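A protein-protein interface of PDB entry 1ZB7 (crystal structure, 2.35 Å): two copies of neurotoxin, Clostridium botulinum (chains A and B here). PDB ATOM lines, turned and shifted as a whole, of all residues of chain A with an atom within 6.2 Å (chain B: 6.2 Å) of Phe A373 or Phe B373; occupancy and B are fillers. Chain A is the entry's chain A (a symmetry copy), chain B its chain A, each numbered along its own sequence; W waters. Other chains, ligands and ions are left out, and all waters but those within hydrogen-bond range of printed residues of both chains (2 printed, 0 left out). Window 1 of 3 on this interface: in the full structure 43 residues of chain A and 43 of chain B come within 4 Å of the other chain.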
ATOM      1  N   ASP A 262       3.179 -12.723  16.414  1.00  0.00           N
ATOM      2  CA  ASP A 262       2.778 -11.789  15.374  1.00  0.00           C
ATOM      3  C   ASP A 262       1.855 -10.667  15.950  1.00  0.00           C
ATOM      4  O   ASP A 262       0.843 -10.961  16.590  1.00  0.00           O
ATOM      5  CB  ASP A 262       2.086 -12.563  14.258  1.00  0.00           C
ATOM      6  CG  ASP A 262       2.126 -11.841  12.913  1.00  0.00           C
ATOM      7  OD1 ASP A 262       2.218 -10.581  12.858  1.00  0.00           O
ATOM      8  OD2 ASP A 262       2.020 -12.570  11.898  1.00  0.00           O
ATOM      9  N   PRO A 263       2.217  -9.388  15.766  1.00  0.00           N
ATOM     10  CA  PRO A 263       1.304  -8.304  16.176  1.00  0.00           C
ATOM     11  C   PRO A 263      -0.062  -8.382  15.524  1.00  0.00           C
ATOM     12  O   PRO A 263      -1.041  -7.949  16.111  1.00  0.00           O
ATOM     13  CB  PRO A 263       2.031  -7.024  15.717  1.00  0.00           C
ATOM     14  CG  PRO A 263       3.463  -7.446  15.683  1.00  0.00           C
ATOM     15  CD  PRO A 263       3.471  -8.852  15.204  1.00  0.00           C
ATOM     16  N   VAL A 264      -0.129  -8.986  14.338  1.00  0.00           N
ATOM     17  CA  VAL A 264      -1.370  -9.013  13.577  1.00  0.00           C
ATOM     18  C   VAL A 264      -1.875 -10.428  13.534  1.00  0.00           C
ATOM     19  O   VAL A 264      -1.562 -11.148  12.635  1.00  0.00           O
ATOM     20  CB  VAL A 264      -1.179  -8.456  12.112  1.00  0.00           C
ATOM     21  CG1 VAL A 264      -2.518  -8.312  11.446  1.00  0.00           C
ATOM     22  CG2 VAL A 264      -0.523  -7.068  12.139  1.00  0.00           C
ATOM     23  N   LEU A 269      -8.439 -10.347  13.528  1.00  0.00           N
ATOM     24  CA  LEU A 269      -8.934  -9.713  12.343  1.00  0.00           C
ATOM     25  C   LEU A 269     -10.203 -10.360  11.782  1.00  0.00           C
ATOM     26  O   LEU A 269     -11.088  -9.641  11.300  1.00  0.00           O
ATOM     27  CB  LEU A 269      -7.847  -9.628  11.283  1.00  0.00           C
ATOM     28  CG  LEU A 269      -6.931  -8.420  11.514  1.00  0.00           C
ATOM     29  CD1 LEU A 269      -5.545  -8.734  11.254  1.00  0.00           C
ATOM     30  CD2 LEU A 269      -7.320  -7.367  10.581  1.00  0.00           C
ATOM     31  N   ASP A 276      -9.426 -10.468   5.402  1.00  0.00           N
ATOM     32  CA  ASP A 276      -8.808  -9.194   5.250  1.00  0.00           C
ATOM     33  C   ASP A 276      -7.553  -9.412   4.450  1.00  0.00           C
ATOM     34  O   ASP A 276      -6.451  -9.413   5.043  1.00  0.00           O
ATOM     35  CB  ASP A 276      -8.528  -8.590   6.630  1.00  0.00           C
ATOM     36  CG  ASP A 276      -8.192  -7.106   6.549  1.00  0.00           C
ATOM     37  OD1 ASP A 276      -8.014  -6.515   7.615  1.00  0.00           O
ATOM     38  OD2 ASP A 276      -8.105  -6.524   5.434  1.00  0.00           O
ATOM     39  N   SER A 278      -5.762  -7.793   2.369  1.00  0.00           N
ATOM     40  CA  SER A 278      -4.798  -6.737   2.259  1.00  0.00           C
ATOM     41  C   SER A 278      -3.870  -6.779   3.456  1.00  0.00           C
ATOM     42  O   SER A 278      -2.810  -6.142   3.396  1.00  0.00           O
ATOM     43  CB  SER A 278      -5.458  -5.345   2.187  1.00  0.00           C
ATOM     44  OG  SER A 278      -5.848  -4.854   3.478  1.00  0.00           O
ATOM     45  N   VAL A 279      -4.296  -7.481   4.525  1.00  0.00           N
ATOM     46  CA  VAL A 279      -3.524  -7.639   5.739  1.00  0.00           C
ATOM     47  C   VAL A 279      -3.096  -9.117   5.990  1.00  0.00           C
ATOM     48  O   VAL A 279      -1.944  -9.357   6.301  1.00  0.00           O
ATOM     49  CB  VAL A 279      -4.299  -7.003   6.926  1.00  0.00           C
ATOM     50  CG1 VAL A 279      -3.827  -7.473   8.252  1.00  0.00           C
ATOM     51  CG2 VAL A 279      -4.099  -5.525   6.892  1.00  0.00           C
ATOM     52  N   ARG A 369     -16.217   1.242  14.393  1.00  0.00           N
ATOM     53  CA  ARG A 369     -15.004   1.710  13.789  1.00  0.00           C
ATOM     54  C   ARG A 369     -14.878   1.188  12.385  1.00  0.00           C
ATOM     55  O   ARG A 369     -15.312   0.096  12.038  1.00  0.00           O
ATOM     56  CB  ARG A 369     -13.833   1.131  14.510  1.00  0.00           C
ATOM     57  CG  ARG A 369     -13.698   1.521  15.938  1.00  0.00           C
ATOM     58  CD  ARG A 369     -12.427   0.973  16.506  1.00  0.00           C
ATOM     59  NE  ARG A 369     -12.305  -0.469  16.450  1.00  0.00           N
ATOM     60  CZ  ARG A 369     -11.144  -1.128  16.564  1.00  0.00           C
ATOM     61  NH1 ARG A 369      -9.955  -0.468  16.641  1.00  0.00           N
ATOM     62  NH2 ARG A 369     -11.182  -2.439  16.569  1.00  0.00           N
ATOM     63  N   SER A 371     -12.120   0.480  10.709  1.00  0.00           N
ATOM     64  CA  SER A 371     -11.249  -0.681  10.663  1.00  0.00           C
ATOM     65  C   SER A 371     -10.655  -1.109  12.005  1.00  0.00           C
ATOM     66  O   SER A 371     -10.763  -0.466  13.050  1.00  0.00           O
ATOM     67  CB  SER A 371     -10.180  -0.472   9.579  1.00  0.00           C
ATOM     68  OG  SER A 371      -8.912  -0.255  10.070  1.00  0.00           O
ATOM     69  N   TYR A 372     -10.092  -2.293  11.961  1.00  0.00           N
ATOM     70  CA  TYR A 372      -9.432  -2.879  13.097  1.00  0.00           C
ATOM     71  C   TYR A 372      -8.252  -2.022  13.548  1.00  0.00           C
ATOM     72  O   TYR A 372      -7.882  -2.011  14.705  1.00  0.00           O
ATOM     73  CB  TYR A 372      -8.973  -4.263  12.658  1.00  0.00           C
ATOM     74  CG  TYR A 372      -8.175  -4.980  13.691  1.00  0.00           C
ATOM     75  CD1 TYR A 372      -8.806  -5.702  14.693  1.00  0.00           C
ATOM     76  CD2 TYR A 372      -6.794  -4.929  13.673  1.00  0.00           C
ATOM     77  CE1 TYR A 372      -8.063  -6.343  15.654  1.00  0.00           C
ATOM     78  CE2 TYR A 372      -6.056  -5.541  14.624  1.00  0.00           C
ATOM     79  CZ  TYR A 372      -6.701  -6.242  15.603  1.00  0.00           C
ATOM     80  OH  TYR A 372      -5.982  -6.863  16.510  1.00  0.00           O
ATOM     81  N   PHE A 373      -7.631  -1.328  12.617  1.00  0.00           N
ATOM     82  CA  PHE A 373      -6.567  -0.395  12.953  1.00  0.00           C
ATOM     83  C   PHE A 373      -7.001   1.068  13.394  1.00  0.00           C
ATOM     84  O   PHE A 373      -6.165   1.905  13.689  1.00  0.00           O
ATOM     85  CB  PHE A 373      -5.552  -0.369  11.783  1.00  0.00           C
ATOM     86  CG  PHE A 373      -5.019  -1.698  11.451  1.00  0.00           C
ATOM     87  CD1 PHE A 373      -3.996  -2.238  12.190  1.00  0.00           C
ATOM     88  CD2 PHE A 373      -5.576  -2.453  10.412  1.00  0.00           C
ATOM     89  CE1 PHE A 373      -3.483  -3.538  11.877  1.00  0.00           C
ATOM     90  CE2 PHE A 373      -5.132  -3.754  10.126  1.00  0.00           C
ATOM     91  CZ  PHE A 373      -4.085  -4.304  10.864  1.00  0.00           C
ATOM     92  N   SER A 374      -8.282   1.377  13.443  1.00  0.00           N
ATOM     93  CA  SER A 374      -8.747   2.712  13.839  1.00  0.00           C
ATOM     94  C   SER A 374      -8.468   2.927  15.307  1.00  0.00           C
ATOM     95  O   SER A 374      -8.714   2.041  16.115  1.00  0.00           O
ATOM     96  CB  SER A 374     -10.271   2.801  13.651  1.00  0.00           C
ATOM     97  OG  SER A 374     -10.689   2.530  12.313  1.00  0.00           O
ATOM     98  N   GLU A 375      -8.063   4.102  15.720  1.00  0.00           N
ATOM     99  CA  GLU A 375      -7.817   4.222  17.144  1.00  0.00           C
ATOM    100  C   GLU A 375      -9.074   4.618  17.956  1.00  0.00           C
ATOM    101  O   GLU A 375      -9.989   5.270  17.457  1.00  0.00           O
ATOM    102  CB  GLU A 375      -6.649   5.145  17.451  1.00  0.00           C
ATOM    103  CG  GLU A 375      -6.775   6.459  16.884  1.00  0.00           C
ATOM    104  CD  GLU A 375      -5.941   7.471  17.642  1.00  0.00           C
ATOM    105  OE1 GLU A 375      -6.519   8.506  18.027  1.00  0.00           O
ATOM    106  OE2 GLU A 375      -4.729   7.210  17.850  1.00  0.00           O
ATOM    107  N   ASP B 262      -3.163  11.213  13.231  1.00  0.00           N
ATOM    108  CA  ASP B 262      -3.635   9.871  12.935  1.00  0.00           C
ATOM    109  C   ASP B 262      -2.440   8.875  12.775  1.00  0.00           C
ATOM    110  O   ASP B 262      -1.524   9.125  11.988  1.00  0.00           O
ATOM    111  CB  ASP B 262      -4.495   9.917  11.677  1.00  0.00           C
ATOM    112  CG  ASP B 262      -5.478   8.754  11.578  1.00  0.00           C
ATOM    113  OD1 ASP B 262      -5.234   7.650  12.148  1.00  0.00           O
ATOM    114  OD2 ASP B 262      -6.496   8.956  10.874  1.00  0.00           O
ATOM    115  N   PRO B 263      -2.421   7.774  13.542  1.00  0.00           N
ATOM    116  CA  PRO B 263      -1.383   6.750  13.324  1.00  0.00           C
ATOM    117  C   PRO B 263      -1.365   6.196  11.913  1.00  0.00           C
ATOM    118  O   PRO B 263      -0.317   5.795  11.430  1.00  0.00           O
ATOM    119  CB  PRO B 263      -1.760   5.634  14.319  1.00  0.00           C
ATOM    120  CG  PRO B 263      -2.527   6.366  15.370  1.00  0.00           C
ATOM    121  CD  PRO B 263      -3.312   7.409  14.659  1.00  0.00           C
ATOM    122  N   VAL B 264      -2.514   6.230  11.239  1.00  0.00           N
ATOM    123  CA  VAL B 264      -2.631   5.621   9.921  1.00  0.00           C
ATOM    124  C   VAL B 264      -2.819   6.713   8.905  1.00  0.00           C
ATOM    125  O   VAL B 264      -3.918   7.064   8.600  1.00  0.00           O
ATOM    126  CB  VAL B 264      -3.827   4.594   9.849  1.00  0.00           C
ATOM    127  CG1 VAL B 264      -3.775   3.847   8.546  1.00  0.00           C
ATOM    128  CG2 VAL B 264      -3.727   3.559  10.979  1.00  0.00           C
ATOM    129  N   LEU B 269       0.074   4.911   3.294  1.00  0.00           N
ATOM    130  CA  LEU B 269      -0.561   3.749   2.749  1.00  0.00           C
ATOM    131  C   LEU B 269      -0.657   3.756   1.222  1.00  0.00           C
ATOM    132  O   LEU B 269      -0.494   2.699   0.599  1.00  0.00           O
ATOM    133  CB  LEU B 269      -1.926   3.533   3.384  1.00  0.00           C
ATOM    134  CG  LEU B 269      -1.811   2.808   4.730  1.00  0.00           C
ATOM    135  CD1 LEU B 269      -2.725   3.343   5.713  1.00  0.00           C
ATOM    136  CD2 LEU B 269      -2.166   1.406   4.526  1.00  0.00           C
ATOM    137  N   ASP B 276      -6.509   1.486  -0.163  1.00  0.00           N
ATOM    138  CA  ASP B 276      -6.576   0.470   0.833  1.00  0.00           C
ATOM    139  C   ASP B 276      -7.870   0.670   1.571  1.00  0.00           C
ATOM    140  O   ASP B 276      -7.844   1.199   2.704  1.00  0.00           O
ATOM    141  CB  ASP B 276      -5.353   0.570   1.751  1.00  0.00           C
ATOM    142  CG  ASP B 276      -5.180  -0.675   2.611  1.00  0.00           C
ATOM    143  OD1 ASP B 276      -4.186  -0.717   3.338  1.00  0.00           O
ATOM    144  OD2 ASP B 276      -6.023  -1.611   2.569  1.00  0.00           O
ATOM    145  N   SER B 278     -10.018  -1.116   3.107  1.00  0.00           N
ATOM    146  CA  SER B 278     -10.257  -1.833   4.326  1.00  0.00           C
ATOM    147  C   SER B 278      -9.647  -1.070   5.483  1.00  0.00           C
ATOM    148  O   SER B 278      -9.995  -1.373   6.633  1.00  0.00           O
ATOM    149  CB  SER B 278      -9.664  -3.255   4.296  1.00  0.00           C
ATOM    150  OG  SER B 278      -8.254  -3.268   4.565  1.00  0.00           O
ATOM    151  N   VAL B 279      -8.726  -0.135   5.171  1.00  0.00           N
ATOM    152  CA  VAL B 279      -8.062   0.695   6.154  1.00  0.00           C
ATOM    153  C   VAL B 279      -8.423   2.204   6.005  1.00  0.00           C
ATOM    154  O   VAL B 279      -8.723   2.843   6.997  1.00  0.00           O
ATOM    155  CB  VAL B 279      -6.535   0.411   6.118  1.00  0.00           C
ATOM    156  CG1 VAL B 279      -5.726   1.481   6.752  1.00  0.00           C
ATOM    157  CG2 VAL B 279      -6.264  -0.846   6.874  1.00  0.00           C
ATOM    158  N   ARG B 369       7.276  -6.948   1.546  1.00  0.00           N
ATOM    159  CA  ARG B 369       6.348  -7.282   2.587  1.00  0.00           C
ATOM    160  C   ARG B 369       4.949  -7.357   2.043  1.00  0.00           C
ATOM    161  O   ARG B 369       4.553  -6.653   1.120  1.00  0.00           O
ATOM    162  CB  ARG B 369       6.302  -6.176   3.587  1.00  0.00           C
ATOM    163  CG  ARG B 369       7.573  -5.908   4.310  1.00  0.00           C
ATOM    164  CD  ARG B 369       7.359  -4.864   5.360  1.00  0.00           C
ATOM    165  NE  ARG B 369       6.878  -3.590   4.868  1.00  0.00           N
ATOM    166  CZ  ARG B 369       6.295  -2.661   5.635  1.00  0.00           C
ATOM    167  NH1 ARG B 369       6.012  -2.896   6.947  1.00  0.00           N
ATOM    168  NH2 ARG B 369       5.970  -1.519   5.077  1.00  0.00           N
ATOM    169  N   SER B 371       2.113  -6.685   3.600  1.00  0.00           N
ATOM    170  CA  SER B 371       1.386  -5.456   3.867  1.00  0.00           C
ATOM    171  C   SER B 371       2.167  -4.385   4.628  1.00  0.00           C
ATOM    172  O   SER B 371       3.282  -4.556   5.124  1.00  0.00           O
ATOM    173  CB  SER B 371       0.041  -5.794   4.528  1.00  0.00           C
ATOM    174  OG  SER B 371      -0.036  -5.454   5.860  1.00  0.00           O
ATOM    175  N   TYR B 372       1.571  -3.216   4.621  1.00  0.00           N
ATOM    176  CA  TYR B 372       2.104  -2.071   5.311  1.00  0.00           C
ATOM    177  C   TYR B 372       2.200  -2.331   6.812  1.00  0.00           C
ATOM    178  O   TYR B 372       3.034  -1.777   7.498  1.00  0.00           O
ATOM    179  CB  TYR B 372       1.161  -0.913   5.010  1.00  0.00           C
ATOM    180  CG  TYR B 372       1.510   0.340   5.732  1.00  0.00           C
ATOM    181  CD1 TYR B 372       2.459   1.211   5.215  1.00  0.00           C
ATOM    182  CD2 TYR B 372       0.903   0.651   6.934  1.00  0.00           C
ATOM    183  CE1 TYR B 372       2.790   2.356   5.898  1.00  0.00           C
ATOM    184  CE2 TYR B 372       1.235   1.765   7.621  1.00  0.00           C
ATOM    185  CZ  TYR B 372       2.176   2.604   7.093  1.00  0.00           C
ATOM    186  OH  TYR B 372       2.477   3.703   7.747  1.00  0.00           O
ATOM    187  N   PHE B 373       1.310  -3.150   7.332  1.00  0.00           N
ATOM    188  CA  PHE B 373       1.378  -3.553   8.728  1.00  0.00           C
ATOM    189  C   PHE B 373       2.332  -4.773   9.083  1.00  0.00           C
ATOM    190  O   PHE B 373       2.439  -5.168  10.231  1.00  0.00           O
ATOM    191  CB  PHE B 373      -0.065  -3.780   9.242  1.00  0.00           C
ATOM    192  CG  PHE B 373      -0.935  -2.608   9.060  1.00  0.00           C
ATOM    193  CD1 PHE B 373      -0.890  -1.568   9.955  1.00  0.00           C
ATOM    194  CD2 PHE B 373      -1.782  -2.511   7.950  1.00  0.00           C
ATOM    195  CE1 PHE B 373      -1.726  -0.420   9.774  1.00  0.00           C
ATOM    196  CE2 PHE B 373      -2.565  -1.369   7.718  1.00  0.00           C
ATOM    197  CZ  PHE B 373      -2.534  -0.314   8.629  1.00  0.00           C
ATOM    198  N   SER B 374       3.017  -5.362   8.121  1.00  0.00           N
ATOM    199  CA  SER B 374       3.911  -6.494   8.384  1.00  0.00           C
ATOM    200  C   SER B 374       5.108  -6.018   9.172  1.00  0.00           C
ATOM    201  O   SER B 374       5.678  -4.981   8.860  1.00  0.00           O
ATOM    202  CB  SER B 374       4.442  -7.049   7.050  1.00  0.00           C
ATOM    203  OG  SER B 374       3.404  -7.461   6.160  1.00  0.00           O
ATOM    204  N   GLU B 375       5.594  -6.775  10.124  1.00  0.00           N
ATOM    205  CA  GLU B 375       6.742  -6.243  10.832  1.00  0.00           C
ATOM    206  C   GLU B 375       8.096  -6.594  10.167  1.00  0.00           C
ATOM    207  O   GLU B 375       8.239  -7.607   9.486  1.00  0.00           O
ATOM    208  CB  GLU B 375       6.738  -6.621  12.304  1.00  0.00           C
ATOM    209  CG  GLU B 375       6.651  -8.035  12.546  1.00  0.00           C
ATOM    210  CD  GLU B 375       7.203  -8.397  13.909  1.00  0.00           C
ATOM    211  OE1 GLU B 375       8.060  -9.302  13.951  1.00  0.00           O
ATOM    212  OE2 GLU B 375       6.781  -7.766  14.911  1.00  0.00           O
HETATM  213  O   HOH W   1      -8.299  -6.225   2.892  1.00  0.00           O
HETATM  214  O   HOH W   2      -8.045  -2.947   1.722  1.00  0.00           O
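Pro A263 touches Glu B375, and with the chains exchanged Glu A375 touches Pro B263. Asp A276 touches Ser B278, and with the chains exchanged Ser A278 touches Asp B276. Ser B278 touches its own counterpart, Ser A278. Ser A278 touches Ser B371, and with the chains exchanged Ser A371 touches Ser B278. Positions printed for both chains: 262, 263, 264, 269, 276, 278, 279, 369, 371, 372, 373, 374 and 375. Of the 10 pairs that touch across the chains among the printed residues, 10 have their exchanged pair printed and touching as well.
Water W2 lies within hydrogen-bond range of the side-chain carboxylate of Asp B276 (2.6 Å), the side-chain hydroxyl of Ser B278 (2.9 Å) and the side-chain hydroxyl of Ser A278 (3.4 Å). Water W1 lies within hydrogen-bond range of OD2 of Asp A276 (2.6 Å), OG of Ser A278 (2.9 Å) and OG of Ser B278 (3.4 Å).
Of the printed residues of chain B, Phe A373 touches Val B279 and Phe B373. Of the printed residues of chain A, Phe B373 touches Val A279 (3.9 Å) and Phe A373 (3.8 Å). Of the printed residues of chain B, Asp A276 touches Ser B278. Of the printed residues of chain A, Asp B276 touches Ser A278 (3.4 Å). Printed residues of chain A within 4 Å of Ser B278: Asp A276, Ser A278 and Ser A371. Of the printed residues of chain A, Glu B375 touches Pro A263 (3.4 Å). The nearest printed residue of chain B that does not touch Phe A373 is Val B264 (4.003 Å).
Among the printed residues, pairs that only touch across the chains: Ser A371 with Ser B278 (3.1 Å), Ser A278 with Ser B371 (3.1 Å), Pro A263 with Glu B375 (3.4 Å), Glu A375 with Pro B263 (3.4 Å), Phe A373 with Phe B373 (3.8 Å), Val A279 with Phe B373 (3.9 Å) and Phe A373 with Val B279 (3.9 Å).
Of the 13 printed residues of chain A, 7 touch a printed residue of chain B. Hydrophobic or aromatic side chains of chain A within 4 Å of the printed part of chain B: Pro A263, Val A279 and Phe A373. Printed residues of chain B that touch a printed residue of chain A: Pro B263, Asp B276, Ser B278, Val B279, Ser B371, Phe B373 and Glu B375. Hydrophobic or aromatic side chains of chain B within 4 Å of the printed part of chain A: Pro B263, Val B279 and Phe B373. Among the printed residues, 10 pairs touch across the chains.
The side-chain carboxylate (OD2) of Asp B276 lies within hydrogen-bond range of the side-chain hydroxyl (OG) of Ser A278 (3.4 Å). The side-chain hydroxyl of Ser B278 is in hydrogen-bond range of the side-chain carboxylate of Asp A276. The side-chain hydroxyl of Ser A278 lies within hydrogen-bond range of the side-chain hydroxyl of Ser B278 (3.1 Å).
The side-chain hydroxyl (OG) of Ser B278 sits at hydrogen-bond distance from the side-chain carboxylate (OD2) of Asp B276 (3.4 Å). The side-chain hydroxyl of Ser B371 is in hydrogen-bond range of the backbone NH of Phe B373, 3.0 Å away. The side-chain hydroxyl of Ser B374 is in hydrogen-bond range of the backbone NH of Ser B371, 3.0 Å away. OG of Ser A278 sits at hydrogen-bond distance from OD2 of Asp A276, 3.4 Å away. The backbone NH (N) of Phe A373 lies within hydrogen-bond range of the side-chain hydroxyl (OG) of Ser A371 (3.0 Å). The side-chain hydroxyl (OG) of Ser A374 is in hydrogen-bond range of the backbone NH (N) of Ser A371, at 3.0 Å.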
